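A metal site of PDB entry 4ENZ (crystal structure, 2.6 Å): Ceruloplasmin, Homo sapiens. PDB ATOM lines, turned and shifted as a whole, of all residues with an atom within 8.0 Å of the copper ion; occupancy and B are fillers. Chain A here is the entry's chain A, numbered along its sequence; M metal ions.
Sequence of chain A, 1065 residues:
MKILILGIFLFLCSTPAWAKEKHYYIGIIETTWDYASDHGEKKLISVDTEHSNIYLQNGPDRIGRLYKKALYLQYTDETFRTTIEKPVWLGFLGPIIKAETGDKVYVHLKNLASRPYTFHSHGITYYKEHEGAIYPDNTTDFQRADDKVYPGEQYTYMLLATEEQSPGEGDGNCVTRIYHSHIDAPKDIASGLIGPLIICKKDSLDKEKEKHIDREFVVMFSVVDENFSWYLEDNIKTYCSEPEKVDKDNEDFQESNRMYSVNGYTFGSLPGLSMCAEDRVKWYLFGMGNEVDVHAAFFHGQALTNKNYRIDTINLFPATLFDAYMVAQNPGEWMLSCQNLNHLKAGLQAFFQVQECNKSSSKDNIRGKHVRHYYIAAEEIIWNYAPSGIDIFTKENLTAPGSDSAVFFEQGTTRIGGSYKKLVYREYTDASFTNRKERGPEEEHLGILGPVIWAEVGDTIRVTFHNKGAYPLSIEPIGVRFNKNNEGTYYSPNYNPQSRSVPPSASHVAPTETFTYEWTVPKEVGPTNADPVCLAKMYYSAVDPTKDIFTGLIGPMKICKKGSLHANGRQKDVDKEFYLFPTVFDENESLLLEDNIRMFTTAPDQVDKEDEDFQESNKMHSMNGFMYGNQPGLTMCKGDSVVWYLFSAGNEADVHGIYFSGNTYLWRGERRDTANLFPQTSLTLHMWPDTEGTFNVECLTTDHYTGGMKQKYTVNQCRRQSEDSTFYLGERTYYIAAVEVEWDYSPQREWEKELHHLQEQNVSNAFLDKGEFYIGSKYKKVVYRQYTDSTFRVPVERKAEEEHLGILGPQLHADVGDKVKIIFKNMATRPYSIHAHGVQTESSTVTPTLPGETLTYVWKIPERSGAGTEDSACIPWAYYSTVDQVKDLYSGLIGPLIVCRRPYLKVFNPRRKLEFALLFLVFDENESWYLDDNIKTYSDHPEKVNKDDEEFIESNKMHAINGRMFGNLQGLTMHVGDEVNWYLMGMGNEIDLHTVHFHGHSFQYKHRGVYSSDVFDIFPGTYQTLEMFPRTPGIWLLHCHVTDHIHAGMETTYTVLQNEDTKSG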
ATOM      1  N   PRO A 582      34.711 -26.461   5.441  1.00  0.00           N
ATOM      2  CA  PRO A 582      33.412 -26.960   5.183  1.00  0.00           C
ATOM      3  C   PRO A 582      33.332 -27.510   3.774  1.00  0.00           C
ATOM      4  O   PRO A 582      33.862 -26.885   2.810  1.00  0.00           O
ATOM      5  CB  PRO A 582      32.546 -25.708   5.278  1.00  0.00           C
ATOM      6  CG  PRO A 582      33.431 -24.614   4.776  1.00  0.00           C
ATOM      7  CD  PRO A 582      34.855 -25.054   5.038  1.00  0.00           C
ATOM      8  N   THR A 583      32.680 -28.656   3.638  1.00  0.00           N
ATOM      9  CA  THR A 583      32.437 -29.210   2.332  1.00  0.00           C
ATOM     10  C   THR A 583      31.374 -30.275   2.393  1.00  0.00           C
ATOM     11  O   THR A 583      30.962 -30.690   3.480  1.00  0.00           O
ATOM     12  CB  THR A 583      33.690 -29.849   1.753  1.00  0.00           C
ATOM     13  OG1 THR A 583      33.387 -30.371   0.450  1.00  0.00           O
ATOM     14  CG2 THR A 583      34.186 -30.982   2.661  1.00  0.00           C
ATOM     15  N   VAL A 584      30.919 -30.704   1.229  1.00  0.00           N
ATOM     16  CA  VAL A 584      30.057 -31.856   1.137  1.00  0.00           C
ATOM     17  C   VAL A 584      30.961 -33.054   0.871  1.00  0.00           C
ATOM     18  O   VAL A 584      31.536 -33.173  -0.243  1.00  0.00           O
ATOM     19  CB  VAL A 584      29.034 -31.703   0.020  1.00  0.00           C
ATOM     20  CG1 VAL A 584      28.059 -32.835   0.065  1.00  0.00           C
ATOM     21  CG2 VAL A 584      28.325 -30.378   0.110  1.00  0.00           C
ATOM     22  N   HIS A 621      27.455 -33.394   4.679  1.00  0.00           N
ATOM     23  CA  HIS A 621      27.615 -31.970   4.778  1.00  0.00           C
ATOM     24  C   HIS A 621      28.197 -31.628   6.113  1.00  0.00           C
ATOM     25  O   HIS A 621      27.522 -31.776   7.140  1.00  0.00           O
ATOM     26  CB  HIS A 621      26.251 -31.304   4.697  1.00  0.00           C
ATOM     27  CG  HIS A 621      25.589 -31.413   3.349  1.00  0.00           C
ATOM     28  ND1 HIS A 621      24.942 -32.553   2.941  1.00  0.00           N
ATOM     29  CD2 HIS A 621      25.464 -30.518   2.347  1.00  0.00           C
ATOM     30  CE1 HIS A 621      24.448 -32.350   1.737  1.00  0.00           C
ATOM     31  NE2 HIS A 621      24.741 -31.117   1.347  1.00  0.00           N
ATOM     32  N   SER A 622      29.409 -31.084   6.110  1.00  0.00           N
ATOM     33  CA  SER A 622      30.226 -31.129   7.297  1.00  0.00           C
ATOM     34  C   SER A 622      31.272 -30.018   7.360  1.00  0.00           C
ATOM     35  O   SER A 622      31.560 -29.399   6.358  1.00  0.00           O
ATOM     36  CB  SER A 622      30.908 -32.522   7.352  1.00  0.00           C
ATOM     37  OG  SER A 622      31.738 -32.756   6.208  1.00  0.00           O
ATOM     38  N   MET A 623      31.808 -29.802   8.571  1.00  0.00           N
ATOM     39  CA  MET A 623      32.934 -28.902   8.843  1.00  0.00           C
ATOM     40  C   MET A 623      34.053 -29.749   9.503  1.00  0.00           C
ATOM     41  O   MET A 623      33.842 -30.358  10.559  1.00  0.00           O
ATOM     42  CB  MET A 623      32.528 -27.767   9.799  1.00  0.00           C
ATOM     43  CG  MET A 623      32.410 -26.373   9.198  1.00  0.00           C
ATOM     44  SD  MET A 623      30.835 -25.484   9.620  1.00  0.00           S
ATOM     45  CE  MET A 623      29.555 -26.608   9.082  1.00  0.00           C
ATOM     46  N   SER A 648      37.698 -24.377   1.188  1.00  0.00           N
ATOM     47  CA  SER A 648      36.816 -25.453   0.772  1.00  0.00           C
ATOM     48  C   SER A 648      37.316 -26.097  -0.509  1.00  0.00           C
ATOM     49  O   SER A 648      38.210 -25.604  -1.165  1.00  0.00           O
ATOM     50  CB  SER A 648      35.380 -24.934   0.567  1.00  0.00           C
ATOM     51  OG  SER A 648      34.476 -26.006   0.310  1.00  0.00           O
ATOM     52  N   ALA A 653      27.973 -27.930  -5.978  1.00  0.00           N
ATOM     53  CA  ALA A 653      27.165 -27.939  -4.747  1.00  0.00           C
ATOM     54  C   ALA A 653      27.838 -27.128  -3.630  1.00  0.00           C
ATOM     55  O   ALA A 653      27.206 -26.763  -2.641  1.00  0.00           O
ATOM     56  CB  ALA A 653      26.904 -29.386  -4.287  1.00  0.00           C
ATOM     57  N   ASP A 654      29.132 -26.865  -3.802  1.00  0.00           N
ATOM     58  CA  ASP A 654      29.924 -26.231  -2.763  1.00  0.00           C
ATOM     59  C   ASP A 654      29.940 -24.722  -2.905  1.00  0.00           C
ATOM     60  O   ASP A 654      30.953 -24.136  -3.252  1.00  0.00           O
ATOM     61  CB  ASP A 654      31.343 -26.792  -2.778  1.00  0.00           C
ATOM     62  CG  ASP A 654      31.377 -28.261  -2.334  1.00  0.00           C
ATOM     63  OD1 ASP A 654      31.353 -28.490  -1.092  1.00  0.00           O
ATOM     64  OD2 ASP A 654      31.424 -29.169  -3.201  1.00  0.00           O
ATOM     65  N   VAL A 655      28.785 -24.100  -2.651  1.00  0.00           N
ATOM     66  CA  VAL A 655      28.707 -22.658  -2.511  1.00  0.00           C
ATOM     67  C   VAL A 655      28.243 -22.407  -1.077  1.00  0.00           C
ATOM     68  O   VAL A 655      27.156 -22.832  -0.664  1.00  0.00           O
ATOM     69  CB  VAL A 655      27.796 -21.971  -3.571  1.00  0.00           C
ATOM     70  CG1 VAL A 655      27.655 -22.850  -4.808  1.00  0.00           C
ATOM     71  CG2 VAL A 655      26.450 -21.578  -2.988  1.00  0.00           C
ATOM     72  N   HIS A 656      29.128 -21.779  -0.300  1.00  0.00           N
ATOM     73  CA  HIS A 656      29.016 -21.848   1.135  1.00  0.00           C
ATOM     74  C   HIS A 656      28.955 -20.441   1.588  1.00  0.00           C
ATOM     75  O   HIS A 656      29.620 -19.603   0.966  1.00  0.00           O
ATOM     76  CB  HIS A 656      30.251 -22.477   1.750  1.00  0.00           C
ATOM     77  CG  HIS A 656      30.431 -23.923   1.428  1.00  0.00           C
ATOM     78  ND1 HIS A 656      29.648 -24.904   1.981  1.00  0.00           N
ATOM     79  CD2 HIS A 656      31.330 -24.544   0.632  1.00  0.00           C
ATOM     80  CE1 HIS A 656      30.045 -26.084   1.518  1.00  0.00           C
ATOM     81  NE2 HIS A 656      31.069 -25.895   0.708  1.00  0.00           N
ATOM     82  N   GLY A 657      28.184 -20.192   2.644  1.00  0.00           N
ATOM     83  CA  GLY A 657      28.177 -18.914   3.338  1.00  0.00           C
ATOM     84  C   GLY A 657      28.361 -19.138   4.837  1.00  0.00           C
ATOM     85  O   GLY A 657      27.374 -19.282   5.540  1.00  0.00           O
ATOM     86  N   ILE A 658      29.610 -19.151   5.318  1.00  0.00           N
ATOM     87  CA  ILE A 658      29.929 -19.530   6.669  1.00  0.00           C
ATOM     88  C   ILE A 658      29.694 -18.353   7.581  1.00  0.00           C
ATOM     89  O   ILE A 658      30.435 -17.392   7.562  1.00  0.00           O
ATOM     90  CB  ILE A 658      31.382 -19.994   6.794  1.00  0.00           C
ATOM     91  CG1 ILE A 658      31.671 -21.103   5.785  1.00  0.00           C
ATOM     92  CG2 ILE A 658      31.677 -20.496   8.195  1.00  0.00           C
ATOM     93  CD1 ILE A 658      30.671 -22.218   5.831  1.00  0.00           C
ATOM     94  N   ALA A 675      31.223 -15.656   5.523  1.00  0.00           N
ATOM     95  CA  ALA A 675      32.322 -15.836   4.562  1.00  0.00           C
ATOM     96  C   ALA A 675      31.874 -16.698   3.400  1.00  0.00           C
ATOM     97  O   ALA A 675      31.382 -17.803   3.627  1.00  0.00           O
ATOM     98  CB  ALA A 675      33.468 -16.484   5.256  1.00  0.00           C
ATOM     99  N   LEU A 677      32.489 -19.237   0.224  1.00  0.00           N
ATOM    100  CA  LEU A 677      33.520 -20.188  -0.186  1.00  0.00           C
ATOM    101  C   LEU A 677      33.048 -21.121  -1.272  1.00  0.00           C
ATOM    102  O   LEU A 677      31.865 -21.485  -1.328  1.00  0.00           O
ATOM    103  CB  LEU A 677      33.947 -21.040   0.984  1.00  0.00           C
ATOM    104  CG  LEU A 677      34.786 -20.301   2.031  1.00  0.00           C
ATOM    105  CD1 LEU A 677      34.793 -21.149   3.258  1.00  0.00           C
ATOM    106  CD2 LEU A 677      36.178 -20.099   1.526  1.00  0.00           C
ATOM    107  N   GLU A 698      27.992 -21.678  11.207  1.00  0.00           N
ATOM    108  CA  GLU A 698      27.127 -22.519  10.407  1.00  0.00           C
ATOM    109  C   GLU A 698      27.106 -22.035   8.988  1.00  0.00           C
ATOM    110  O   GLU A 698      27.356 -20.855   8.734  1.00  0.00           O
ATOM    111  CB  GLU A 698      25.728 -22.456  10.975  1.00  0.00           C
ATOM    112  CG  GLU A 698      25.041 -21.110  10.704  1.00  0.00           C
ATOM    113  CD  GLU A 698      23.774 -20.898  11.548  1.00  0.00           C
ATOM    114  OE1 GLU A 698      23.680 -21.450  12.655  1.00  0.00           O
ATOM    115  OE2 GLU A 698      22.891 -20.149  11.080  1.00  0.00           O
ATOM    116  N   CYS A 699      26.789 -22.931   8.059  1.00  0.00           N
ATOM    117  CA  CYS A 699      26.561 -22.522   6.669  1.00  0.00           C
ATOM    118  C   CYS A 699      25.128 -22.016   6.461  1.00  0.00           C
ATOM    119  O   CYS A 699      24.177 -22.694   6.783  1.00  0.00           O
ATOM    120  CB  CYS A 699      26.877 -23.645   5.681  1.00  0.00           C
ATOM    121  SG  CYS A 699      26.962 -23.020   3.995  1.00  0.00           S
ATOM    122  N   LEU A 700      25.019 -20.801   5.979  1.00  0.00           N
ATOM    123  CA  LEU A 700      23.740 -20.179   5.659  1.00  0.00           C
ATOM    124  C   LEU A 700      22.990 -20.905   4.525  1.00  0.00           C
ATOM    125  O   LEU A 700      21.755 -20.855   4.477  1.00  0.00           O
ATOM    126  CB  LEU A 700      23.966 -18.717   5.202  1.00  0.00           C
ATOM    127  CG  LEU A 700      23.769 -17.713   6.310  1.00  0.00           C
ATOM    128  CD1 LEU A 700      24.250 -16.330   5.905  1.00  0.00           C
ATOM    129  CD2 LEU A 700      22.285 -17.713   6.658  1.00  0.00           C
ATOM    130  N   THR A 701      23.733 -21.514   3.590  1.00  0.00           N
ATOM    131  CA  THR A 701      23.122 -22.114   2.408  1.00  0.00           C
ATOM    132  C   THR A 701      22.166 -23.197   2.866  1.00  0.00           C
ATOM    133  O   THR A 701      22.501 -24.110   3.604  1.00  0.00           O
ATOM    134  CB  THR A 701      24.148 -22.677   1.417  1.00  0.00           C
ATOM    135  OG1 THR A 701      24.840 -23.713   2.098  1.00  0.00           O
ATOM    136  CG2 THR A 701      25.169 -21.647   1.038  1.00  0.00           C
ATOM    137  N   THR A 702      20.939 -23.051   2.412  1.00  0.00           N
ATOM    138  CA  THR A 702      19.784 -23.759   2.956  1.00  0.00           C
ATOM    139  C   THR A 702      19.948 -25.256   3.142  1.00  0.00           C
ATOM    140  O   THR A 702      19.775 -25.777   4.263  1.00  0.00           O
ATOM    141  CB  THR A 702      18.596 -23.349   2.113  1.00  0.00           C
ATOM    142  OG1 THR A 702      17.991 -22.250   2.817  1.00  0.00           O
ATOM    143  CG2 THR A 702      17.609 -24.529   1.802  1.00  0.00           C
ATOM    144  N   ASP A 703      20.321 -25.953   2.064  1.00  0.00           N
ATOM    145  CA  ASP A 703      20.512 -27.392   2.169  1.00  0.00           C
ATOM    146  C   ASP A 703      21.719 -27.802   3.002  1.00  0.00           C
ATOM    147  O   ASP A 703      21.664 -28.849   3.670  1.00  0.00           O
ATOM    148  CB  ASP A 703      20.576 -28.045   0.790  1.00  0.00           C
ATOM    149  CG  ASP A 703      19.180 -28.129   0.108  1.00  0.00           C
ATOM    150  OD1 ASP A 703      18.123 -27.886   0.787  1.00  0.00           O
ATOM    151  OD2 ASP A 703      19.153 -28.426  -1.113  1.00  0.00           O
ATOM    152  N   HIS A 704      22.781 -26.992   2.999  1.00  0.00           N
ATOM    153  CA  HIS A 704      23.920 -27.331   3.846  1.00  0.00           C
ATOM    154  C   HIS A 704      23.505 -27.296   5.317  1.00  0.00           C
ATOM    155  O   HIS A 704      23.856 -28.165   6.099  1.00  0.00           O
ATOM    156  CB  HIS A 704      25.138 -26.430   3.607  1.00  0.00           C
ATOM    157  CG  HIS A 704      25.625 -26.396   2.190  1.00  0.00           C
ATOM    158  ND1 HIS A 704      26.657 -25.587   1.780  1.00  0.00           N
ATOM    159  CD2 HIS A 704      25.193 -27.051   1.079  1.00  0.00           C
ATOM    160  CE1 HIS A 704      26.858 -25.760   0.479  1.00  0.00           C
ATOM    161  NE2 HIS A 704      25.974 -26.635   0.035  1.00  0.00           N
ATOM    162  N   TYR A 705      22.692 -26.323   5.684  1.00  0.00           N
ATOM    163  CA  TYR A 705      22.286 -26.198   7.078  1.00  0.00           C
ATOM    164  C   TYR A 705      21.392 -27.394   7.477  1.00  0.00           C
ATOM    165  O   TYR A 705      21.693 -28.113   8.413  1.00  0.00           O
ATOM    166  CB  TYR A 705      21.597 -24.835   7.320  1.00  0.00           C
ATOM    167  CG  TYR A 705      21.188 -24.639   8.754  1.00  0.00           C
ATOM    168  CD1 TYR A 705      22.097 -24.143   9.702  1.00  0.00           C
ATOM    169  CD2 TYR A 705      19.941 -24.999   9.182  1.00  0.00           C
ATOM    170  CE1 TYR A 705      21.751 -23.986  11.056  1.00  0.00           C
ATOM    171  CE2 TYR A 705      19.559 -24.823  10.546  1.00  0.00           C
ATOM    172  CZ  TYR A 705      20.478 -24.334  11.477  1.00  0.00           C
ATOM    173  OH  TYR A 705      20.083 -24.170  12.789  1.00  0.00           O
ATOM    174  N   MET A 709      25.510 -28.892   8.353  1.00  0.00           N
ATOM    175  CA  MET A 709      26.731 -28.082   8.285  1.00  0.00           C
ATOM    176  C   MET A 709      26.575 -26.966   9.293  1.00  0.00           C
ATOM    177  O   MET A 709      26.348 -25.840   8.931  1.00  0.00           O
ATOM    178  CB  MET A 709      26.974 -27.538   6.861  1.00  0.00           C
ATOM    179  CG  MET A 709      28.439 -27.156   6.471  1.00  0.00           C
ATOM    180  SD  MET A 709      28.653 -26.533   4.732  1.00  0.00           S
ATOM    181  CE  MET A 709      28.460 -28.160   3.891  1.00  0.00           C
ATOM    182  N   GLU A 990      22.189 -23.797  -2.666  1.00  0.00           N
ATOM    183  CA  GLU A 990      23.339 -24.037  -3.590  1.00  0.00           C
ATOM    184  C   GLU A 990      23.178 -23.281  -4.905  1.00  0.00           C
ATOM    185  O   GLU A 990      24.116 -22.752  -5.466  1.00  0.00           O
ATOM    186  CB  GLU A 990      23.432 -25.547  -3.911  1.00  0.00           C
ATOM    187  CG  GLU A 990      23.783 -26.406  -2.692  1.00  0.00           C
ATOM    188  CD  GLU A 990      23.713 -27.925  -2.918  1.00  0.00           C
ATOM    189  OE1 GLU A 990      23.189 -28.387  -3.960  1.00  0.00           O
ATOM    190  OE2 GLU A 990      24.211 -28.655  -2.006  1.00  0.00           O
HETATM  191 CU    CU M   1      27.884 -24.638   2.863  1.00  0.00          CU
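ND1 of His 704 sits close to OG1 of Thr 701 (2.6 Å).
The backbone carbonyl oxygen (O) of Ala 653 lies within hydrogen-bond range of a ring nitrogen (NE2) of His 704 (2.9 Å).
OE2 of Glu 990 is in hydrogen-bond range of NE2 of His 704.
The side-chain carboxylate (OD1) of Asp 654 is in hydrogen-bond range of a ring nitrogen (NE2) of His 656, 3.2 Å away.
The backbone NH of His 656 sits at hydrogen-bond distance from the backbone carbonyl oxygen of Leu 677 (2.9 Å).
The side-chain hydroxyl of Ser 648 sits at hydrogen-bond distance from a ring nitrogen (NE2) of His 656 (3.4 Å).
OG1 of Thr 701 lies close to SG of Cys 699 (2.9 Å).
SG of Cys 699 sits close to N of Gly 657 (3.4 Å).
Thr 701 touches the copper ion (OG1 to CU, 3.3 Å).
Of the 25 residues printed, 5 come within 4 Å of the copper ion.
The nearest printed residue that does not touch the copper ion is Val 655 (4.03 Å).
A ring nitrogen (ND1) of His 704 is bound to the copper ion (1.9 Å).
The copper ion is bound by ND1 of His 656 (2.0 Å).
The copper ion is bound by the side-chain sulfur (SG) of Cys 699 (2.2 Å).
The side-chain sulfur (SD) of Met 709 binds the copper ion, 2.8 Å away.
The copper ion has four donor atoms within binding distance.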
